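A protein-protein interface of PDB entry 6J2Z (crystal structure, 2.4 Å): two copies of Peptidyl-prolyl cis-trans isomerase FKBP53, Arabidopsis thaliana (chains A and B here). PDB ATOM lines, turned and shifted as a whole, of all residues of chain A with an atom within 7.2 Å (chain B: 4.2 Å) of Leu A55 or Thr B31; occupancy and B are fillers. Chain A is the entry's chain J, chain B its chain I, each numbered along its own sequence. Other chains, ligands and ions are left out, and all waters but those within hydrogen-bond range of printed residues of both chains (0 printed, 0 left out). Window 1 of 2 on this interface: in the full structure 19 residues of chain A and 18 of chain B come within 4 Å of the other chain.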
ATOM      1  N   VAL A  27      -6.923 -10.956  12.538  1.00  0.00           N
ATOM      2  CA  VAL A  27      -6.282 -11.957  13.431  1.00  0.00           C
ATOM      3  C   VAL A  27      -5.765 -13.071  12.528  1.00  0.00           C
ATOM      4  O   VAL A  27      -6.609 -13.689  11.823  1.00  0.00           O
ATOM      5  CB  VAL A  27      -7.259 -12.489  14.487  1.00  0.00           C
ATOM      6  CG1 VAL A  27      -6.541 -13.403  15.469  1.00  0.00           C
ATOM      7  CG2 VAL A  27      -7.937 -11.339  15.225  1.00  0.00           C
ATOM      8  N   ALA A  30      -2.690 -17.653  16.242  1.00  0.00           N
ATOM      9  CA  ALA A  30      -2.765 -17.974  17.680  1.00  0.00           C
ATOM     10  C   ALA A  30      -1.479 -18.700  18.074  1.00  0.00           C
ATOM     11  O   ALA A  30      -1.075 -19.638  17.347  1.00  0.00           O
ATOM     12  CB  ALA A  30      -3.980 -18.815  17.959  1.00  0.00           C
ATOM     13  N   VAL A  42      -7.820 -24.345  23.917  1.00  0.00           N
ATOM     14  CA  VAL A  42      -8.838 -23.954  22.901  1.00  0.00           C
ATOM     15  C   VAL A  42      -9.224 -22.502  23.176  1.00  0.00           C
ATOM     16  O   VAL A  42      -9.444 -22.175  24.352  1.00  0.00           O
ATOM     17  CB  VAL A  42     -10.070 -24.875  22.955  1.00  0.00           C
ATOM     18  CG1 VAL A  42     -11.138 -24.455  21.954  1.00  0.00           C
ATOM     19  CG2 VAL A  42      -9.689 -26.332  22.769  1.00  0.00           C
ATOM     20  N   ILE A  43      -9.282 -21.669  22.140  1.00  0.00           N
ATOM     21  CA  ILE A  43      -9.827 -20.293  22.259  1.00  0.00           C
ATOM     22  C   ILE A  43     -11.165 -20.252  21.523  1.00  0.00           C
ATOM     23  O   ILE A  43     -11.244 -20.724  20.370  1.00  0.00           O
ATOM     24  CB  ILE A  43      -8.857 -19.194  21.784  1.00  0.00           C
ATOM     25  CG1 ILE A  43      -9.487 -17.809  21.955  1.00  0.00           C
ATOM     26  CG2 ILE A  43      -8.380 -19.422  20.356  1.00  0.00           C
ATOM     27  CD1 ILE A  43      -8.489 -16.691  21.939  1.00  0.00           C
ATOM     28  N   GLN A  44     -12.184 -19.744  22.214  1.00  0.00           N
ATOM     29  CA  GLN A  44     -13.557 -19.567  21.696  1.00  0.00           C
ATOM     30  C   GLN A  44     -13.869 -18.077  21.624  1.00  0.00           C
ATOM     31  O   GLN A  44     -13.256 -17.283  22.354  1.00  0.00           O
ATOM     32  CB  GLN A  44     -14.569 -20.243  22.610  1.00  0.00           C
ATOM     33  CG  GLN A  44     -14.547 -21.757  22.530  1.00  0.00           C
ATOM     34  CD  GLN A  44     -15.374 -22.324  23.652  1.00  0.00           C
ATOM     35  OE1 GLN A  44     -14.928 -22.380  24.799  1.00  0.00           O
ATOM     36  NE2 GLN A  44     -16.596 -22.721  23.327  1.00  0.00           N
ATOM     37  N   CYS A  45     -14.840 -17.749  20.787  1.00  0.00           N
ATOM     38  CA  CYS A  45     -15.289 -16.374  20.496  1.00  0.00           C
ATOM     39  C   CYS A  45     -16.813 -16.352  20.520  1.00  0.00           C
ATOM     40  O   CYS A  45     -17.425 -17.176  19.858  1.00  0.00           O
ATOM     41  CB  CYS A  45     -14.749 -15.938  19.146  1.00  0.00           C
ATOM     42  SG  CYS A  45     -15.352 -14.304  18.670  1.00  0.00           S
ATOM     43  N   SER A  46     -17.404 -15.461  21.306  1.00  0.00           N
ATOM     44  CA  SER A  46     -18.853 -15.152  21.289  1.00  0.00           C
ATOM     45  C   SER A  46     -19.045 -13.690  20.879  1.00  0.00           C
ATOM     46  O   SER A  46     -18.306 -12.835  21.391  1.00  0.00           O
ATOM     47  CB  SER A  46     -19.452 -15.457  22.631  1.00  0.00           C
ATOM     48  OG  SER A  46     -20.850 -15.224  22.639  1.00  0.00           O
ATOM     49  N   ILE A  53     -18.001 -19.974  19.563  1.00  0.00           N
ATOM     50  CA  ILE A  53     -17.449 -20.795  18.441  1.00  0.00           C
ATOM     51  C   ILE A  53     -15.947 -20.957  18.693  1.00  0.00           C
ATOM     52  O   ILE A  53     -15.270 -19.935  18.934  1.00  0.00           O
ATOM     53  CB  ILE A  53     -17.732 -20.123  17.083  1.00  0.00           C
ATOM     54  CG1 ILE A  53     -19.232 -19.909  16.842  1.00  0.00           C
ATOM     55  CG2 ILE A  53     -17.055 -20.884  15.962  1.00  0.00           C
ATOM     56  CD1 ILE A  53     -20.007 -21.175  16.552  1.00  0.00           C
ATOM     57  N   ALA A  54     -15.448 -22.191  18.634  1.00  0.00           N
ATOM     58  CA  ALA A  54     -14.006 -22.507  18.777  1.00  0.00           C
ATOM     59  C   ALA A  54     -13.276 -21.996  17.535  1.00  0.00           C
ATOM     60  O   ALA A  54     -13.754 -22.257  16.410  1.00  0.00           O
ATOM     61  CB  ALA A  54     -13.791 -23.987  19.001  1.00  0.00           C
ATOM     62  N   LEU A  55     -12.188 -21.253  17.745  1.00  0.00           N
ATOM     63  CA  LEU A  55     -11.401 -20.600  16.668  1.00  0.00           C
ATOM     64  C   LEU A  55     -10.196 -21.464  16.307  1.00  0.00           C
ATOM     65  O   LEU A  55      -9.744 -21.367  15.155  1.00  0.00           O
ATOM     66  CB  LEU A  55     -10.909 -19.249  17.170  1.00  0.00           C
ATOM     67  CG  LEU A  55     -12.005 -18.254  17.547  1.00  0.00           C
ATOM     68  CD1 LEU A  55     -11.379 -16.911  17.893  1.00  0.00           C
ATOM     69  CD2 LEU A  55     -13.023 -18.091  16.421  1.00  0.00           C
ATOM     70  N   CYS A  56      -9.652 -22.192  17.285  1.00  0.00           N
ATOM     71  CA  CYS A  56      -8.533 -23.137  17.094  1.00  0.00           C
ATOM     72  C   CYS A  56      -8.235 -23.868  18.403  1.00  0.00           C
ATOM     73  O   CYS A  56      -8.827 -23.539  19.441  1.00  0.00           O
ATOM     74  CB  CYS A  56      -7.272 -22.430  16.614  1.00  0.00           C
ATOM     75  SG  CYS A  56      -6.643 -21.261  17.835  1.00  0.00           S
ATOM     76  N   SER A  57      -7.318 -24.819  18.314  1.00  0.00           N
ATOM     77  CA  SER A  57      -6.982 -25.821  19.342  1.00  0.00           C
ATOM     78  C   SER A  57      -5.485 -26.084  19.228  1.00  0.00           C
ATOM     79  O   SER A  57      -5.057 -26.556  18.166  1.00  0.00           O
ATOM     80  CB  SER A  57      -7.805 -27.060  19.137  1.00  0.00           C
ATOM     81  OG  SER A  57      -7.672 -27.944  20.240  1.00  0.00           O
ATOM     82  N   LEU A  58      -4.722 -25.683  20.246  1.00  0.00           N
ATOM     83  CA  LEU A  58      -3.247 -25.825  20.296  1.00  0.00           C
ATOM     84  C   LEU A  58      -2.897 -26.961  21.251  1.00  0.00           C
ATOM     85  O   LEU A  58      -3.569 -27.089  22.286  1.00  0.00           O
ATOM     86  CB  LEU A  58      -2.638 -24.488  20.730  1.00  0.00           C
ATOM     87  CG  LEU A  58      -2.911 -23.327  19.771  1.00  0.00           C
ATOM     88  CD1 LEU A  58      -2.198 -22.088  20.222  1.00  0.00           C
ATOM     89  CD2 LEU A  58      -2.479 -23.649  18.347  1.00  0.00           C
ATOM     90  N   CYS A  66      -0.908 -21.675  15.246  1.00  0.00           N
ATOM     91  CA  CYS A  66      -1.690 -22.002  14.030  1.00  0.00           C
ATOM     92  C   CYS A  66      -2.096 -20.727  13.322  1.00  0.00           C
ATOM     93  O   CYS A  66      -2.384 -19.712  13.954  1.00  0.00           O
ATOM     94  CB  CYS A  66      -2.915 -22.843  14.346  1.00  0.00           C
ATOM     95  SG  CYS A  66      -4.094 -21.986  15.411  1.00  0.00           S
ATOM     96  N   PRO A  67      -2.083 -20.751  11.976  1.00  0.00           N
ATOM     97  CA  PRO A  67      -2.497 -19.600  11.189  1.00  0.00           C
ATOM     98  C   PRO A  67      -4.020 -19.420  11.303  1.00  0.00           C
ATOM     99  O   PRO A  67      -4.739 -20.394  11.380  1.00  0.00           O
ATOM    100  CB  PRO A  67      -2.037 -19.940   9.770  1.00  0.00           C
ATOM    101  CG  PRO A  67      -2.040 -21.453   9.740  1.00  0.00           C
ATOM    102  CD  PRO A  67      -1.684 -21.886  11.150  1.00  0.00           C
ATOM    103  N   LEU A  68      -4.458 -18.168  11.386  1.00  0.00           N
ATOM    104  CA  LEU A  68      -5.891 -17.798  11.398  1.00  0.00           C
ATOM    105  C   LEU A  68      -6.127 -16.799  10.269  1.00  0.00           C
ATOM    106  O   LEU A  68      -5.151 -16.230   9.766  1.00  0.00           O
ATOM    107  CB  LEU A  68      -6.268 -17.173  12.741  1.00  0.00           C
ATOM    108  CG  LEU A  68      -6.115 -18.074  13.959  1.00  0.00           C
ATOM    109  CD1 LEU A  68      -6.287 -17.279  15.252  1.00  0.00           C
ATOM    110  CD2 LEU A  68      -7.097 -19.243  13.889  1.00  0.00           C
ATOM    111  N   LEU A  70      -9.166 -14.172  10.485  1.00  0.00           N
ATOM    112  CA  LEU A  70     -10.407 -13.602  11.054  1.00  0.00           C
ATOM    113  C   LEU A  70     -10.361 -12.080  10.915  1.00  0.00           C
ATOM    114  O   LEU A  70      -9.261 -11.495  10.927  1.00  0.00           O
ATOM    115  CB  LEU A  70     -10.543 -14.025  12.521  1.00  0.00           C
ATOM    116  CG  LEU A  70     -10.610 -15.534  12.769  1.00  0.00           C
ATOM    117  CD1 LEU A  70     -10.643 -15.787  14.275  1.00  0.00           C
ATOM    118  CD2 LEU A  70     -11.806 -16.200  12.101  1.00  0.00           C
ATOM    119  N   PHE A  72     -12.370  -8.694  12.600  1.00  0.00           N
ATOM    120  CA  PHE A  72     -13.240  -8.015  13.591  1.00  0.00           C
ATOM    121  C   PHE A  72     -13.309  -6.534  13.226  1.00  0.00           C
ATOM    122  O   PHE A  72     -12.257  -5.925  12.964  1.00  0.00           O
ATOM    123  CB  PHE A  72     -12.725  -8.264  15.006  1.00  0.00           C
ATOM    124  CG  PHE A  72     -12.760  -9.715  15.408  1.00  0.00           C
ATOM    125  CD1 PHE A  72     -13.938 -10.306  15.837  1.00  0.00           C
ATOM    126  CD2 PHE A  72     -11.625 -10.504  15.305  1.00  0.00           C
ATOM    127  CE1 PHE A  72     -13.965 -11.639  16.211  1.00  0.00           C
ATOM    128  CE2 PHE A  72     -11.654 -11.844  15.673  1.00  0.00           C
ATOM    129  CZ  PHE A  72     -12.826 -12.406  16.132  1.00  0.00           C
ATOM    130  N   GLU A  80     -16.308 -11.627  23.074  1.00  0.00           N
ATOM    131  CA  GLU A  80     -15.840 -12.321  24.300  1.00  0.00           C
ATOM    132  C   GLU A  80     -14.957 -13.504  23.887  1.00  0.00           C
ATOM    133  O   GLU A  80     -15.454 -14.401  23.199  1.00  0.00           O
ATOM    134  CB  GLU A  80     -17.033 -12.740  25.155  1.00  0.00           C
ATOM    135  CG  GLU A  80     -16.682 -13.008  26.598  1.00  0.00           C
ATOM    136  CD  GLU A  80     -17.907 -13.242  27.465  1.00  0.00           C
ATOM    137  OE1 GLU A  80     -18.695 -12.291  27.680  1.00  0.00           O
ATOM    138  OE2 GLU A  80     -18.085 -14.382  27.915  1.00  0.00           O
ATOM    139  N   PHE A  81     -13.681 -13.453  24.246  1.00  0.00           N
ATOM    140  CA  PHE A  81     -12.705 -14.554  24.057  1.00  0.00           C
ATOM    141  C   PHE A  81     -12.647 -15.381  25.337  1.00  0.00           C
ATOM    142  O   PHE A  81     -12.524 -14.797  26.429  1.00  0.00           O
ATOM    143  CB  PHE A  81     -11.331 -14.008  23.683  1.00  0.00           C
ATOM    144  CG  PHE A  81     -11.270 -13.389  22.313  1.00  0.00           C
ATOM    145  CD1 PHE A  81     -11.611 -14.130  21.193  1.00  0.00           C
ATOM    146  CD2 PHE A  81     -10.855 -12.082  22.138  1.00  0.00           C
ATOM    147  CE1 PHE A  81     -11.534 -13.571  19.925  1.00  0.00           C
ATOM    148  CE2 PHE A  81     -10.775 -11.524  20.870  1.00  0.00           C
ATOM    149  CZ  PHE A  81     -11.140 -12.263  19.761  1.00  0.00           C
ATOM    150  N   LEU A  91      -2.945 -13.943  20.447  1.00  0.00           N
ATOM    151  CA  LEU A  91      -3.452 -13.582  19.097  1.00  0.00           C
ATOM    152  C   LEU A  91      -2.566 -12.468  18.537  1.00  0.00           C
ATOM    153  O   LEU A  91      -2.223 -11.545  19.285  1.00  0.00           O
ATOM    154  CB  LEU A  91      -4.918 -13.140  19.186  1.00  0.00           C
ATOM    155  CG  LEU A  91      -5.879 -14.162  19.796  1.00  0.00           C
ATOM    156  CD1 LEU A  91      -7.259 -13.552  19.944  1.00  0.00           C
ATOM    157  CD2 LEU A  91      -5.922 -15.439  18.966  1.00  0.00           C
ATOM    158  N   PHE B   3     -17.348 -10.947  12.033  1.00  0.00           N
ATOM    159  CA  PHE B   3     -17.071 -12.335  12.465  1.00  0.00           C
ATOM    160  C   PHE B   3     -18.232 -13.224  12.020  1.00  0.00           C
ATOM    161  O   PHE B   3     -19.374 -12.784  12.072  1.00  0.00           O
ATOM    162  CB  PHE B   3     -16.860 -12.453  13.972  1.00  0.00           C
ATOM    163  CG  PHE B   3     -16.668 -13.880  14.420  1.00  0.00           C
ATOM    164  CD1 PHE B   3     -15.457 -14.526  14.230  1.00  0.00           C
ATOM    165  CD2 PHE B   3     -17.707 -14.592  14.999  1.00  0.00           C
ATOM    166  CE1 PHE B   3     -15.283 -15.844  14.627  1.00  0.00           C
ATOM    167  CE2 PHE B   3     -17.532 -15.911  15.397  1.00  0.00           C
ATOM    168  CZ  PHE B   3     -16.321 -16.536  15.207  1.00  0.00           C
ATOM    169  N   GLN B  29     -11.312 -21.382   8.923  1.00  0.00           N
ATOM    170  CA  GLN B  29     -10.820 -22.332   9.946  1.00  0.00           C
ATOM    171  C   GLN B  29     -11.887 -23.380  10.252  1.00  0.00           C
ATOM    172  O   GLN B  29     -13.093 -23.036  10.273  1.00  0.00           O
ATOM    173  CB  GLN B  29     -10.461 -21.573  11.222  1.00  0.00           C
ATOM    174  CG  GLN B  29      -9.611 -22.371  12.202  1.00  0.00           C
ATOM    175  CD  GLN B  29      -8.140 -22.402  11.876  1.00  0.00           C
ATOM    176  OE1 GLN B  29      -7.402 -23.221  12.403  1.00  0.00           O
ATOM    177  NE2 GLN B  29      -7.685 -21.509  11.014  1.00  0.00           N
ATOM    178  N   ALA B  30     -11.446 -24.611  10.486  1.00  0.00           N
ATOM    179  CA  ALA B  30     -12.218 -25.684  11.149  1.00  0.00           C
ATOM    180  C   ALA B  30     -11.506 -26.037  12.458  1.00  0.00           C
ATOM    181  O   ALA B  30     -10.259 -26.217  12.438  1.00  0.00           O
ATOM    182  CB  ALA B  30     -12.326 -26.882  10.243  1.00  0.00           C
ATOM    183  N   THR B  31     -12.261 -26.102  13.553  1.00  0.00           N
ATOM    184  CA  THR B  31     -11.733 -26.436  14.894  1.00  0.00           C
ATOM    185  C   THR B  31     -12.590 -27.557  15.477  1.00  0.00           C
ATOM    186  O   THR B  31     -13.831 -27.491  15.375  1.00  0.00           O
ATOM    187  CB  THR B  31     -11.680 -25.206  15.800  1.00  0.00           C
ATOM    188  OG1 THR B  31     -10.888 -24.222  15.138  1.00  0.00           O
ATOM    189  CG2 THR B  31     -11.078 -25.514  17.154  1.00  0.00           C
ATOM    190  N   LEU B  32     -11.932 -28.543  16.078  1.00  0.00           N
ATOM    191  CA  LEU B  32     -12.586 -29.745  16.636  1.00  0.00           C
ATOM    192  C   LEU B  32     -13.351 -29.333  17.894  1.00  0.00           C
ATOM    193  O   LEU B  32     -12.768 -28.627  18.714  1.00  0.00           O
ATOM    194  CB  LEU B  32     -11.484 -30.764  16.944  1.00  0.00           C
ATOM    195  CG  LEU B  32     -11.958 -32.196  17.138  1.00  0.00           C
ATOM    196  CD1 LEU B  32     -12.752 -32.678  15.944  1.00  0.00           C
ATOM    197  CD2 LEU B  32     -10.775 -33.107  17.399  1.00  0.00           C
ATOM    198  N   GLY B  33     -14.621 -29.718  18.008  1.00  0.00           N
ATOM    199  CA  GLY B  33     -15.436 -29.481  19.213  1.00  0.00           C
ATOM    200  C   GLY B  33     -15.020 -30.387  20.361  1.00  0.00           C
ATOM    201  O   GLY B  33     -14.219 -31.320  20.135  1.00  0.00           O
ATOM    202  N   LEU B  58      -9.597 -33.646  10.798  1.00  0.00           N
ATOM    203  CA  LEU B  58      -8.987 -33.285  12.100  1.00  0.00           C
ATOM    204  C   LEU B  58      -8.762 -34.575  12.894  1.00  0.00           C
ATOM    205  O   LEU B  58      -9.621 -35.486  12.828  1.00  0.00           O
ATOM    206  CB  LEU B  58      -9.904 -32.305  12.838  1.00  0.00           C
ATOM    207  CG  LEU B  58     -10.153 -30.988  12.108  1.00  0.00           C
ATOM    208  CD1 LEU B  58     -11.034 -30.063  12.922  1.00  0.00           C
ATOM    209  CD2 LEU B  58      -8.853 -30.290  11.764  1.00  0.00           C
ATOM    210  N   GLU B  64      -6.066 -30.474  15.717  1.00  0.00           N
ATOM    211  CA  GLU B  64      -7.429 -30.192  16.243  1.00  0.00           C
ATOM    212  C   GLU B  64      -8.003 -28.914  15.616  1.00  0.00           C
ATOM    213  O   GLU B  64      -9.134 -28.529  15.978  1.00  0.00           O
ATOM    214  CB  GLU B  64      -7.381 -30.125  17.759  1.00  0.00           C
ATOM    215  CG  GLU B  64      -7.030 -31.462  18.350  1.00  0.00           C
ATOM    216  CD  GLU B  64      -7.558 -31.720  19.740  1.00  0.00           C
ATOM    217  OE1 GLU B  64      -8.078 -30.771  20.359  1.00  0.00           O
ATOM    218  OE2 GLU B  64      -7.412 -32.876  20.210  1.00  0.00           O
ATOM    219  N   CYS B  65      -7.256 -28.287  14.710  1.00  0.00           N
ATOM    220  CA  CYS B  65      -7.784 -27.205  13.846  1.00  0.00           C
ATOM    221  C   CYS B  65      -6.947 -27.144  12.573  1.00  0.00           C
ATOM    222  O   CYS B  65      -5.853 -27.712  12.563  1.00  0.00           O
ATOM    223  CB  CYS B  65      -7.786 -25.865  14.564  1.00  0.00           C
ATOM    224  SG  CYS B  65      -6.113 -25.298  14.941  1.00  0.00           S
ATOM    225  N   ILE B  89     -17.665 -29.904  14.584  1.00  0.00           N
ATOM    226  CA  ILE B  89     -16.599 -29.080  13.951  1.00  0.00           C
ATOM    227  C   ILE B  89     -17.092 -27.634  13.909  1.00  0.00           C
ATOM    228  O   ILE B  89     -18.190 -27.382  13.374  1.00  0.00           O
ATOM    229  CB  ILE B  89     -16.221 -29.641  12.570  1.00  0.00           C
ATOM    230  CG1 ILE B  89     -15.486 -30.976  12.732  1.00  0.00           C
ATOM    231  CG2 ILE B  89     -15.432 -28.614  11.760  1.00  0.00           C
ATOM    232  CD1 ILE B  89     -14.807 -31.487  11.487  1.00  0.00           C
ATOM    233  N   HIS B  90     -16.325 -26.742  14.532  1.00  0.00           N
ATOM    234  CA  HIS B  90     -16.567 -25.282  14.568  1.00  0.00           C
ATOM    235  C   HIS B  90     -15.915 -24.661  13.337  1.00  0.00           C
ATOM    236  O   HIS B  90     -14.656 -24.644  13.267  1.00  0.00           O
ATOM    237  CB  HIS B  90     -16.002 -24.693  15.864  1.00  0.00           C
ATOM    238  CG  HIS B  90     -16.691 -25.165  17.103  1.00  0.00           C
ATOM    239  ND1 HIS B  90     -17.358 -24.315  17.955  1.00  0.00           N
ATOM    240  CD2 HIS B  90     -16.815 -26.404  17.631  1.00  0.00           C
ATOM    241  CE1 HIS B  90     -17.856 -25.012  18.959  1.00  0.00           C
ATOM    242  NE2 HIS B  90     -17.548 -26.296  18.775  1.00  0.00           N
ATOM    243  N   SER B  92     -15.227 -21.153  11.392  1.00  0.00           N
ATOM    244  CA  SER B  92     -15.108 -19.707  11.695  1.00  0.00           C
ATOM    245  C   SER B  92     -14.569 -18.997  10.458  1.00  0.00           C
ATOM    246  O   SER B  92     -14.014 -19.670   9.563  1.00  0.00           O
ATOM    247  CB  SER B  92     -14.241 -19.482  12.915  1.00  0.00           C
ATOM    248  OG  SER B  92     -12.955 -20.069  12.749  1.00  0.00           O
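2 positions are printed for both chains.
Among the printed residues, merely in contact across the chains: Leu A55 with Gln B29 (3.1 Å), Cys A56 with Cys B65 (3.5 Å), Ile A53 with His B90 (3.6 Å), Ala A54 with Thr B31 (3.6 Å), Leu A55 with Phe B3 (3.7 Å), Leu A68 with Gln B29 (3.7 Å), Phe A72 with Phe B3 (3.7 Å), Cys A66 with Cys B65 (3.9 Å), Leu A55 with Ser B92 (3.96 Å) and Ser A57 with Thr B31 (3.996 Å).
SG of Cys A56 lies close to SG of Cys A66 (3.6 Å).
The backbone carbonyl oxygen of Gln B29 lies within hydrogen-bond range of the backbone NH of Ser B92, at 3.1 Å.
The backbone carbonyl oxygen (O) of Cys A45 is in hydrogen-bond range of the backbone NH (N) of Ile A53, at 2.9 Å.
O of Ala A30 lies within hydrogen-bond range of N of Cys A66 (2.9 Å).
O of Thr B31 is in hydrogen-bond range of N of His B90 (2.7 Å).
The backbone NH of Leu A55 lies within hydrogen-bond range of the backbone carbonyl oxygen of Ile A43 (2.8 Å).
The side-chain amide nitrogen of Gln B29 sits at hydrogen-bond distance from the backbone carbonyl oxygen of Pro A67 (3.2 Å).
The side-chain hydroxyl of Thr B31 is in hydrogen-bond range of the backbone NH of Cys A56 (3.2 Å).
The backbone NH of Ala A54 lies within hydrogen-bond range of a ring nitrogen (ND1) of His B90 (2.9 Å).
SG of Cys B65 lies within hydrogen-bond range of N of Ser A57, 3.6 Å away.
OE1 of Glu B64 sits at hydrogen-bond distance from OG of Ser A57, 2.9 Å away.
The side-chain hydroxyl (OG1) of Thr B31 lies close to the backbone carbonyl oxygen (O) of Leu A55 (3.1 Å).
Hydrophobic or aromatic side chains of chain B within 4 Å of the printed part of chain A: Phe B3 and His B90.
Printed residues of chain A that touch a printed residue of chain B: Ile A53, Ala A54, Leu A55, Cys A56, Ser A57, Cys A66, Pro A67, Leu A68 and Phe A72.
Hydrophobic or aromatic side chains of chain A within 4 Å of the printed part of chain B: Ile A53, Ala A54, Leu A55, Leu A68 and Phe A72.
Among the printed residues, 16 pairs touch across the chains.
Among the printed residues, no Asp or Glu carboxylate lies within 4 Å of a Lys or Arg side-chain nitrogen of the other chain.
Ser A46 touches none of the printed residues of chain B.
Leu A55 touches four residues of chain B.
Printed residues of chain B within 4 Å of Cys A66: Cys B65.
Of the printed residues of chain B, Phe A72 touches Phe B3.
Of the printed residues of chain A, Phe B3 touches Leu A55 (3.7 Å) and Phe A72 (3.7 Å).
Of the printed residues of chain A, Thr B31 touches Ala A54, Leu A55, Cys A56 and Ser A57.
Printed residues of chain A within 4 Å of His B90: Ile A53 and Ala A54.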
